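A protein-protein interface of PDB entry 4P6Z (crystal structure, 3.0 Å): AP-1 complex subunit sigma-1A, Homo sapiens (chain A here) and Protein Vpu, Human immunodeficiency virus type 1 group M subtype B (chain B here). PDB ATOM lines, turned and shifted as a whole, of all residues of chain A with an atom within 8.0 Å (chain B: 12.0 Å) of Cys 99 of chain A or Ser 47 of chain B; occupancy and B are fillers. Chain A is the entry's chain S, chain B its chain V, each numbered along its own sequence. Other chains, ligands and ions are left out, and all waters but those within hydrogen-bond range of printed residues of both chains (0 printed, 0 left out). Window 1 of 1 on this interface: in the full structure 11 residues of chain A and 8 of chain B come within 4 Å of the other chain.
Of chain B, only Glu 45, Leu 46 and Ser 47 come within 4 Å of Cys 99 of chain A.
Of chain A, only Cys 99 comes within 4 Å of Ser 47 of chain B.
No residue of chain B comes within 4 Å of Phe 95 of chain A.
Gly 96 of chain A touches none of the printed residues of chain B.
Val 98 of chain A touches just these residues of chain B: Ala 48 and Leu 49.
Of chain B, only Glu 45 (3.5 Å) comes within 4 Å of Glu 100 of chain A.
Leu 101 of chain A touches just these residues of chain B: Glu 45 and Leu 46.
No residue of chain B comes within 4 Å of Asp 102 of chain A.
Ala 48 of chain B touches just these residues of chain A: Ala 63 (3.8 Å) and Val 98 (3.5 Å).
Printed residues of chain B within 4 Å of Ser 64 of chain A: Glu 44.
Printed residues of chain B within 4 Å of Tyr 62 of chain A: Leu 49 (3.4 Å).
The nearest residue of chain A that does not touch Ser 47 of chain B is Val 98 of chain A (4.1 Å).
Printed residues of chain B that touch a printed residue of chain A: Glu 44, Glu 45, Leu 46, Ser 47, Ala 48 and Leu 49.
Hydrophobic or aromatic side chains of chain B that line the printed part of chain A: Leu 46 and Leu 49.
Hydrophobic or aromatic side chains of chain A within 4 Å of the printed part of chain B: Tyr 62, Ala 63, Phe 67, Val 98 and Leu 101.
The side-chain hydroxyl (OG) of Ser 64 of chain A lies within hydrogen-bond range of the backbone carbonyl oxygen (O) of Glu 44 of chain B, at 3.4 Å.
The backbone NH of Leu 49 of chain B sits at hydrogen-bond distance from the backbone carbonyl oxygen of Val 98 of chain A (2.8 Å).
O of Glu 45 of chain B sits at hydrogen-bond distance from SG of Cys 99 of chain A (3.4 Å).
N of Leu 101 of chain A is in hydrogen-bond range of O of Glu 45 of chain B, 3.1 Å away.
Among the printed residues, merely in contact across the chains: Cys 99 of chain A with Leu 46 of chain B (3.2 Å), Cys 99 of chain A with Ser 47 of chain B (3.2 Å), Tyr 62 of chain A with Leu 49 of chain B (3.4 Å), Val 98 of chain A with Ala 48 of chain B (3.5 Å), Glu 100 of chain A with Glu 45 of chain B (3.5 Å), Leu 101 of chain A with Leu 46 of chain B (3.6 Å), Ala 63 of chain A with Glu 44 of chain B (3.7 Å), Ala 63 of chain A with Ala 48 of chain B (3.8 Å) and Phe 67 of chain A with Leu 49 of chain B (3.9 Å).
OG of Ser 64 of chain A sits at hydrogen-bond distance from OE1 of Glu 100 of chain A, 2.5 Å away.
The side-chain carboxylate (OD1) of Asp 92 of chain A sits at hydrogen-bond distance from the backbone NH (N) of Val 98 of chain A (3.4 Å).
The side-chain sulfur of Cys 99 of chain A lies close to the backbone NH of Leu 101 of chain A (3.4 Å).
The backbone NH (N) of Cys 99 of chain A lies within hydrogen-bond range of the side-chain carboxylate (OD2) of Asp 102 of chain A (3.4 Å).
OD2 of Asp 42 of chain B sits at hydrogen-bond distance from N of Glu 44 of chain B, 2.7 Å away.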
ATOM      1  N   TYR A  62     -24.803  11.157 -29.297  1.00  0.00           N
ATOM      2  CA  TYR A  62     -25.259   9.812 -29.028  1.00  0.00           C
ATOM      3  C   TYR A  62     -26.701   9.905 -28.609  1.00  0.00           C
ATOM      4  O   TYR A  62     -27.048  10.556 -27.597  1.00  0.00           O
ATOM      5  CB  TYR A  62     -24.435   9.189 -27.906  1.00  0.00           C
ATOM      6  CG  TYR A  62     -23.021   8.857 -28.284  1.00  0.00           C
ATOM      7  CD1 TYR A  62     -22.020   9.798 -28.204  1.00  0.00           C
ATOM      8  CD2 TYR A  62     -22.692   7.587 -28.674  1.00  0.00           C
ATOM      9  CE1 TYR A  62     -20.728   9.496 -28.534  1.00  0.00           C
ATOM     10  CE2 TYR A  62     -21.400   7.253 -29.012  1.00  0.00           C
ATOM     11  CZ  TYR A  62     -20.419   8.217 -28.937  1.00  0.00           C
ATOM     12  OH  TYR A  62     -19.113   7.905 -29.224  1.00  0.00           O
ATOM     13  N   ALA A  63     -27.555   9.271 -29.414  1.00  0.00           N
ATOM     14  CA  ALA A  63     -29.030   9.374 -29.247  1.00  0.00           C
ATOM     15  C   ALA A  63     -29.471  10.804 -29.222  1.00  0.00           C
ATOM     16  O   ALA A  63     -29.424  11.502 -30.224  1.00  0.00           O
ATOM     17  CB  ALA A  63     -29.506   8.653 -28.003  1.00  0.00           C
ATOM     18  N   SER A  64     -29.903  11.248 -28.061  1.00  0.00           N
ATOM     19  CA  SER A  64     -30.439  12.599 -27.871  1.00  0.00           C
ATOM     20  C   SER A  64     -29.415  13.453 -27.151  1.00  0.00           C
ATOM     21  O   SER A  64     -29.590  14.653 -27.073  1.00  0.00           O
ATOM     22  CB  SER A  64     -31.664  12.485 -26.983  1.00  0.00           C
ATOM     23  OG  SER A  64     -31.316  11.901 -25.690  1.00  0.00           O
ATOM     24  N   LEU A  65     -28.353  12.829 -26.604  1.00  0.00           N
ATOM     25  CA  LEU A  65     -27.408  13.544 -25.786  1.00  0.00           C
ATOM     26  C   LEU A  65     -26.142  13.915 -26.584  1.00  0.00           C
ATOM     27  O   LEU A  65     -25.527  13.069 -27.257  1.00  0.00           O
ATOM     28  CB  LEU A  65     -27.048  12.691 -24.590  1.00  0.00           C
ATOM     29  CG  LEU A  65     -26.085  13.259 -23.557  1.00  0.00           C
ATOM     30  CD1 LEU A  65     -26.563  14.631 -23.087  1.00  0.00           C
ATOM     31  CD2 LEU A  65     -25.884  12.274 -22.409  1.00  0.00           C
ATOM     32  N   PHE A  67     -22.283  15.111 -26.728  1.00  0.00           N
ATOM     33  CA  PHE A  67     -21.003  15.156 -26.003  1.00  0.00           C
ATOM     34  C   PHE A  67     -20.098  16.101 -26.758  1.00  0.00           C
ATOM     35  O   PHE A  67     -19.900  15.947 -27.989  1.00  0.00           O
ATOM     36  CB  PHE A  67     -20.389  13.782 -25.945  1.00  0.00           C
ATOM     37  CG  PHE A  67     -21.139  12.799 -25.086  1.00  0.00           C
ATOM     38  CD1 PHE A  67     -22.409  12.352 -25.452  1.00  0.00           C
ATOM     39  CD2 PHE A  67     -20.586  12.308 -23.919  1.00  0.00           C
ATOM     40  CE1 PHE A  67     -23.105  11.443 -24.650  1.00  0.00           C
ATOM     41  CE2 PHE A  67     -21.265  11.419 -23.118  1.00  0.00           C
ATOM     42  CZ  PHE A  67     -22.519  10.960 -23.480  1.00  0.00           C
ATOM     43  N   LEU A  91     -19.901   4.781 -19.177  1.00  0.00           N
ATOM     44  CA  LEU A  91     -21.247   5.041 -18.733  1.00  0.00           C
ATOM     45  C   LEU A  91     -22.124   3.843 -19.037  1.00  0.00           C
ATOM     46  O   LEU A  91     -22.915   3.413 -18.170  1.00  0.00           O
ATOM     47  CB  LEU A  91     -21.825   6.291 -19.407  1.00  0.00           C
ATOM     48  CG  LEU A  91     -21.228   7.627 -18.980  1.00  0.00           C
ATOM     49  CD1 LEU A  91     -21.673   8.784 -19.860  1.00  0.00           C
ATOM     50  CD2 LEU A  91     -21.539   7.875 -17.523  1.00  0.00           C
ATOM     51  N   ASP A  92     -21.983   3.298 -20.259  1.00  0.00           N
ATOM     52  CA  ASP A  92     -22.810   2.197 -20.693  1.00  0.00           C
ATOM     53  C   ASP A  92     -22.652   1.012 -19.779  1.00  0.00           C
ATOM     54  O   ASP A  92     -23.634   0.369 -19.418  1.00  0.00           O
ATOM     55  CB  ASP A  92     -22.543   1.835 -22.136  1.00  0.00           C
ATOM     56  CG  ASP A  92     -23.482   0.709 -22.635  1.00  0.00           C
ATOM     57  OD1 ASP A  92     -24.626   0.992 -22.951  1.00  0.00           O
ATOM     58  OD2 ASP A  92     -23.125  -0.483 -22.714  1.00  0.00           O
ATOM     59  N   PHE A  95     -24.059   2.157 -15.809  1.00  0.00           N
ATOM     60  CA  PHE A  95     -25.504   2.189 -15.656  1.00  0.00           C
ATOM     61  C   PHE A  95     -26.180   0.985 -16.285  1.00  0.00           C
ATOM     62  O   PHE A  95     -27.255   0.587 -15.887  1.00  0.00           O
ATOM     63  CB  PHE A  95     -26.075   3.480 -16.255  1.00  0.00           C
ATOM     64  CG  PHE A  95     -25.684   4.713 -15.499  1.00  0.00           C
ATOM     65  CD1 PHE A  95     -24.760   5.586 -16.012  1.00  0.00           C
ATOM     66  CD2 PHE A  95     -26.260   5.011 -14.292  1.00  0.00           C
ATOM     67  CE1 PHE A  95     -24.413   6.736 -15.335  1.00  0.00           C
ATOM     68  CE2 PHE A  95     -25.903   6.141 -13.604  1.00  0.00           C
ATOM     69  CZ  PHE A  95     -24.971   7.004 -14.125  1.00  0.00           C
ATOM     70  N   GLY A  96     -25.560   0.434 -17.311  1.00  0.00           N
ATOM     71  CA  GLY A  96     -26.199  -0.635 -18.072  1.00  0.00           C
ATOM     72  C   GLY A  96     -27.194  -0.111 -19.062  1.00  0.00           C
ATOM     73  O   GLY A  96     -28.228   0.399 -18.678  1.00  0.00           O
ATOM     74  N   SER A  97     -26.852  -0.250 -20.335  1.00  0.00           N
ATOM     75  CA  SER A  97     -27.696   0.235 -21.437  1.00  0.00           C
ATOM     76  C   SER A  97     -28.046   1.690 -21.214  1.00  0.00           C
ATOM     77  O   SER A  97     -29.205   2.050 -21.077  1.00  0.00           O
ATOM     78  CB  SER A  97     -28.941  -0.634 -21.571  1.00  0.00           C
ATOM     79  OG  SER A  97     -29.528  -0.403 -22.815  1.00  0.00           O
ATOM     80  N   VAL A  98     -27.018   2.532 -21.169  1.00  0.00           N
ATOM     81  CA  VAL A  98     -27.155   3.897 -20.672  1.00  0.00           C
ATOM     82  C   VAL A  98     -27.981   4.742 -21.608  1.00  0.00           C
ATOM     83  O   VAL A  98     -27.855   4.618 -22.828  1.00  0.00           O
ATOM     84  CB  VAL A  98     -25.787   4.528 -20.378  1.00  0.00           C
ATOM     85  CG1 VAL A  98     -25.053   4.791 -21.667  1.00  0.00           C
ATOM     86  CG2 VAL A  98     -25.958   5.836 -19.662  1.00  0.00           C
ATOM     87  N   CYS A  99     -28.837   5.578 -21.038  1.00  0.00           N
ATOM     88  CA  CYS A  99     -29.653   6.524 -21.814  1.00  0.00           C
ATOM     89  C   CYS A  99     -29.431   7.906 -21.207  1.00  0.00           C
ATOM     90  O   CYS A  99     -28.831   8.005 -20.118  1.00  0.00           O
ATOM     91  CB  CYS A  99     -31.132   6.156 -21.738  1.00  0.00           C
ATOM     92  SG  CYS A  99     -31.775   6.360 -20.090  1.00  0.00           S
ATOM     93  N   GLU A 100     -29.910   8.954 -21.889  1.00  0.00           N
ATOM     94  CA  GLU A 100     -29.787  10.280 -21.335  1.00  0.00           C
ATOM     95  C   GLU A 100     -30.410  10.419 -19.938  1.00  0.00           C
ATOM     96  O   GLU A 100     -29.835  11.083 -19.055  1.00  0.00           O
ATOM     97  CB  GLU A 100     -30.411  11.313 -22.237  1.00  0.00           C
ATOM     98  CG  GLU A 100     -30.146  12.744 -21.773  1.00  0.00           C
ATOM     99  CD  GLU A 100     -30.836  13.785 -22.598  1.00  0.00           C
ATOM    100  OE1 GLU A 100     -31.355  13.477 -23.691  1.00  0.00           O
ATOM    101  OE2 GLU A 100     -30.839  14.941 -22.162  1.00  0.00           O
ATOM    102  N   LEU A 101     -31.546   9.767 -19.733  1.00  0.00           N
ATOM    103  CA  LEU A 101     -32.238   9.865 -18.469  1.00  0.00           C
ATOM    104  C   LEU A 101     -31.394   9.450 -17.270  1.00  0.00           C
ATOM    105  O   LEU A 101     -31.490  10.061 -16.184  1.00  0.00           O
ATOM    106  CB  LEU A 101     -33.510   8.998 -18.496  1.00  0.00           C
ATOM    107  CG  LEU A 101     -34.582   9.389 -17.446  1.00  0.00           C
ATOM    108  CD1 LEU A 101     -34.894  10.879 -17.494  1.00  0.00           C
ATOM    109  CD2 LEU A 101     -35.803   8.525 -17.748  1.00  0.00           C
ATOM    110  N   ASP A 102     -30.549   8.444 -17.461  1.00  0.00           N
ATOM    111  CA  ASP A 102     -29.641   8.034 -16.398  1.00  0.00           C
ATOM    112  C   ASP A 102     -28.693   9.160 -16.036  1.00  0.00           C
ATOM    113  O   ASP A 102     -28.470   9.432 -14.836  1.00  0.00           O
ATOM    114  CB  ASP A 102     -28.831   6.796 -16.809  1.00  0.00           C
ATOM    115  CG  ASP A 102     -29.705   5.561 -16.968  1.00  0.00           C
ATOM    116  OD1 ASP A 102     -30.704   5.440 -16.247  1.00  0.00           O
ATOM    117  OD2 ASP A 102     -29.433   4.710 -17.823  1.00  0.00           O
ATOM    118  N   ILE A 103     -28.143   9.832 -17.058  1.00  0.00           N
ATOM    119  CA  ILE A 103     -27.272  10.984 -16.815  1.00  0.00           C
ATOM    120  C   ILE A 103     -28.017  12.106 -16.137  1.00  0.00           C
ATOM    121  O   ILE A 103     -27.475  12.746 -15.222  1.00  0.00           O
ATOM    122  CB  ILE A 103     -26.577  11.468 -18.085  1.00  0.00           C
ATOM    123  CG1 ILE A 103     -25.451  10.492 -18.464  1.00  0.00           C
ATOM    124  CG2 ILE A 103     -25.907  12.796 -17.844  1.00  0.00           C
ATOM    125  CD1 ILE A 103     -25.904   9.401 -19.391  1.00  0.00           C
ATOM    126  N   ILE A 104     -29.256  12.306 -16.567  1.00  0.00           N
ATOM    127  CA  ILE A 104     -30.141  13.307 -15.920  1.00  0.00           C
ATOM    128  C   ILE A 104     -30.326  13.068 -14.430  1.00  0.00           C
ATOM    129  O   ILE A 104     -30.238  14.002 -13.673  1.00  0.00           O
ATOM    130  CB  ILE A 104     -31.545  13.327 -16.590  1.00  0.00           C
ATOM    131  CG1 ILE A 104     -31.411  13.680 -18.045  1.00  0.00           C
ATOM    132  CG2 ILE A 104     -32.471  14.271 -15.888  1.00  0.00           C
ATOM    133  CD1 ILE A 104     -32.721  13.885 -18.717  1.00  0.00           C
ATOM    134  N   PHE A 105     -30.579  11.820 -14.038  1.00  0.00           N
ATOM    135  CA  PHE A 105     -30.849  11.514 -12.639  1.00  0.00           C
ATOM    136  C   PHE A 105     -29.644  11.137 -11.831  1.00  0.00           C
ATOM    137  O   PHE A 105     -29.712  11.036 -10.614  1.00  0.00           O
ATOM    138  CB  PHE A 105     -31.871  10.374 -12.548  1.00  0.00           C
ATOM    139  CG  PHE A 105     -33.295  10.826 -12.657  1.00  0.00           C
ATOM    140  CD1 PHE A 105     -33.950  10.781 -13.869  1.00  0.00           C
ATOM    141  CD2 PHE A 105     -33.957  11.336 -11.527  1.00  0.00           C
ATOM    142  CE1 PHE A 105     -35.236  11.232 -13.956  1.00  0.00           C
ATOM    143  CE2 PHE A 105     -35.259  11.794 -11.601  1.00  0.00           C
ATOM    144  CZ  PHE A 105     -35.897  11.743 -12.813  1.00  0.00           C
ATOM    145  N   ASN A 106     -28.534  10.892 -12.508  1.00  0.00           N
ATOM    146  CA  ASN A 106     -27.289  10.470 -11.815  1.00  0.00           C
ATOM    147  C   ASN A 106     -26.097  11.293 -12.195  1.00  0.00           C
ATOM    148  O   ASN A 106     -24.998  10.774 -12.263  1.00  0.00           O
ATOM    149  CB  ASN A 106     -27.019   8.974 -12.030  1.00  0.00           C
ATOM    150  CG  ASN A 106     -28.238   8.155 -11.817  1.00  0.00           C
ATOM    151  OD1 ASN A 106     -28.483   7.688 -10.708  1.00  0.00           O
ATOM    152  ND2 ASN A 106     -29.035   7.996 -12.868  1.00  0.00           N
ATOM    153  N   ASP B  42     -39.015  13.681 -23.434  1.00  0.00           N
ATOM    154  CA  ASP B  42     -39.110  13.050 -24.791  1.00  0.00           C
ATOM    155  C   ASP B  42     -38.840  11.541 -24.725  1.00  0.00           C
ATOM    156  O   ASP B  42     -38.223  11.043 -23.759  1.00  0.00           O
ATOM    157  CB  ASP B  42     -38.113  13.707 -25.748  1.00  0.00           C
ATOM    158  CG  ASP B  42     -38.222  13.177 -27.163  1.00  0.00           C
ATOM    159  OD1 ASP B  42     -39.046  13.686 -27.957  1.00  0.00           O
ATOM    160  OD2 ASP B  42     -37.477  12.231 -27.480  1.00  0.00           O
ATOM    161  N   GLN B  43     -39.292  10.840 -25.763  1.00  0.00           N
ATOM    162  CA  GLN B  43     -39.086   9.413 -25.900  1.00  0.00           C
ATOM    163  C   GLN B  43     -37.593   9.028 -25.935  1.00  0.00           C
ATOM    164  O   GLN B  43     -37.140   8.110 -25.228  1.00  0.00           O
ATOM    165  CB  GLN B  43     -39.804   8.914 -27.147  1.00  0.00           C
ATOM    166  CG  GLN B  43     -39.491   7.468 -27.466  1.00  0.00           C
ATOM    167  CD  GLN B  43     -40.303   6.944 -28.641  1.00  0.00           C
ATOM    168  OE1 GLN B  43     -41.517   7.177 -28.755  1.00  0.00           O
ATOM    169  NE2 GLN B  43     -39.630   6.232 -29.527  1.00  0.00           N
ATOM    170  N   GLU B  44     -36.828   9.741 -26.752  1.00  0.00           N
ATOM    171  CA  GLU B  44     -35.421   9.421 -26.954  1.00  0.00           C
ATOM    172  C   GLU B  44     -34.570   9.601 -25.706  1.00  0.00           C
ATOM    173  O   GLU B  44     -33.413   9.192 -25.670  1.00  0.00           O
ATOM    174  CB  GLU B  44     -34.848  10.246 -28.093  1.00  0.00           C
ATOM    175  CG  GLU B  44     -34.685   9.465 -29.390  1.00  0.00           C
ATOM    176  CD  GLU B  44     -33.372   9.808 -30.091  1.00  0.00           C
ATOM    177  OE1 GLU B  44     -32.647   8.863 -30.567  1.00  0.00           O
ATOM    178  OE2 GLU B  44     -33.070  11.037 -30.116  1.00  0.00           O
ATOM    179  N   GLU B  45     -35.130  10.201 -24.669  1.00  0.00           N
ATOM    180  CA  GLU B  45     -34.445  10.273 -23.384  1.00  0.00           C
ATOM    181  C   GLU B  45     -34.226   8.892 -22.789  1.00  0.00           C
ATOM    182  O   GLU B  45     -33.406   8.730 -21.921  1.00  0.00           O
ATOM    183  CB  GLU B  45     -35.209  11.163 -22.416  1.00  0.00           C
ATOM    184  CG  GLU B  45     -35.104  12.643 -22.652  1.00  0.00           C
ATOM    185  CD  GLU B  45     -35.870  13.414 -21.578  1.00  0.00           C
ATOM    186  OE1 GLU B  45     -36.541  12.734 -20.735  1.00  0.00           O
ATOM    187  OE2 GLU B  45     -35.826  14.696 -21.560  1.00  0.00           O
ATOM    188  N   LEU B  46     -34.992   7.921 -23.257  1.00  0.00           N
ATOM    189  CA  LEU B  46     -34.825   6.537 -22.826  1.00  0.00           C
ATOM    190  C   LEU B  46     -33.969   5.742 -23.775  1.00  0.00           C
ATOM    191  O   LEU B  46     -33.434   4.704 -23.358  1.00  0.00           O
ATOM    192  CB  LEU B  46     -36.158   5.821 -22.667  1.00  0.00           C
ATOM    193  CG  LEU B  46     -36.910   6.059 -21.383  1.00  0.00           C
ATOM    194  CD1 LEU B  46     -38.041   5.071 -21.203  1.00  0.00           C
ATOM    195  CD2 LEU B  46     -35.949   5.932 -20.220  1.00  0.00           C
ATOM    196  N   SER B  47     -33.808   6.236 -25.013  1.00  0.00           N
ATOM    197  CA  SER B  47     -33.036   5.514 -26.004  1.00  0.00           C
ATOM    198  C   SER B  47     -31.590   5.312 -25.582  1.00  0.00           C
ATOM    199  O   SER B  47     -30.963   6.221 -24.977  1.00  0.00           O
ATOM    200  CB  SER B  47     -33.105   6.249 -27.329  1.00  0.00           C
ATOM    201  OG  SER B  47     -34.330   5.997 -27.978  1.00  0.00           O
ATOM    202  N   ALA B  48     -31.052   4.147 -25.950  1.00  0.00           N
ATOM    203  CA  ALA B  48     -29.693   3.749 -25.640  1.00  0.00           C
ATOM    204  C   ALA B  48     -28.724   4.678 -26.327  1.00  0.00           C
ATOM    205  O   ALA B  48     -28.859   4.978 -27.545  1.00  0.00           O
ATOM    206  CB  ALA B  48     -29.448   2.326 -26.122  1.00  0.00           C
ATOM    207  N   LEU B  49     -27.737   5.158 -25.575  1.00  0.00           N
ATOM    208  CA  LEU B  49     -26.687   5.965 -26.166  1.00  0.00           C
ATOM    209  C   LEU B  49     -25.901   5.170 -27.201  1.00  0.00           C
ATOM    210  O   LEU B  49     -25.543   5.701 -28.250  1.00  0.00           O
ATOM    211  CB  LEU B  49     -25.744   6.442 -25.052  1.00  0.00           C
ATOM    212  CG  LEU B  49     -26.282   7.462 -24.062  1.00  0.00           C
ATOM    213  CD1 LEU B  49     -25.059   8.030 -23.334  1.00  0.00           C
ATOM    214  CD2 LEU B  49     -27.014   8.535 -24.839  1.00  0.00           C
ATOM    215  N   VAL B  50     -25.648   3.894 -26.881  1.00  0.00           N
ATOM    216  CA  VAL B  50     -24.772   3.060 -27.667  1.00  0.00           C
ATOM    217  C   VAL B  50     -25.529   2.047 -28.505  1.00  0.00           C
ATOM    218  O   VAL B  50     -25.528   2.127 -29.749  1.00  0.00           O
ATOM    219  CB  VAL B  50     -23.785   2.344 -26.772  1.00  0.00           C
ATOM    220  CG1 VAL B  50     -23.014   1.340 -27.576  1.00  0.00           C
ATOM    221  CG2 VAL B  50     -22.796   3.330 -26.222  1.00  0.00           C
ATOM    222  N   GLU B  51     -26.162   1.090 -27.823  1.00  0.00           N
ATOM    223  CA  GLU B  51     -26.812  -0.038 -28.539  1.00  0.00           C
ATOM    224  C   GLU B  51     -25.899  -0.727 -29.583  1.00  0.00           C
ATOM    225  O   GLU B  51     -25.331  -1.782 -29.323  1.00  0.00           O
ATOM    226  CB  GLU B  51     -28.113   0.439 -29.201  1.00  0.00           C
ATOM    227  CG  GLU B  51     -28.691  -0.580 -30.178  1.00  0.00           C
ATOM    228  CD  GLU B  51     -30.125  -0.954 -29.847  1.00  0.00           C
ATOM    229  OE1 GLU B  51     -30.685  -0.375 -28.871  1.00  0.00           O
ATOM    230  OE2 GLU B  51     -30.681  -1.829 -30.558  1.00  0.00           O
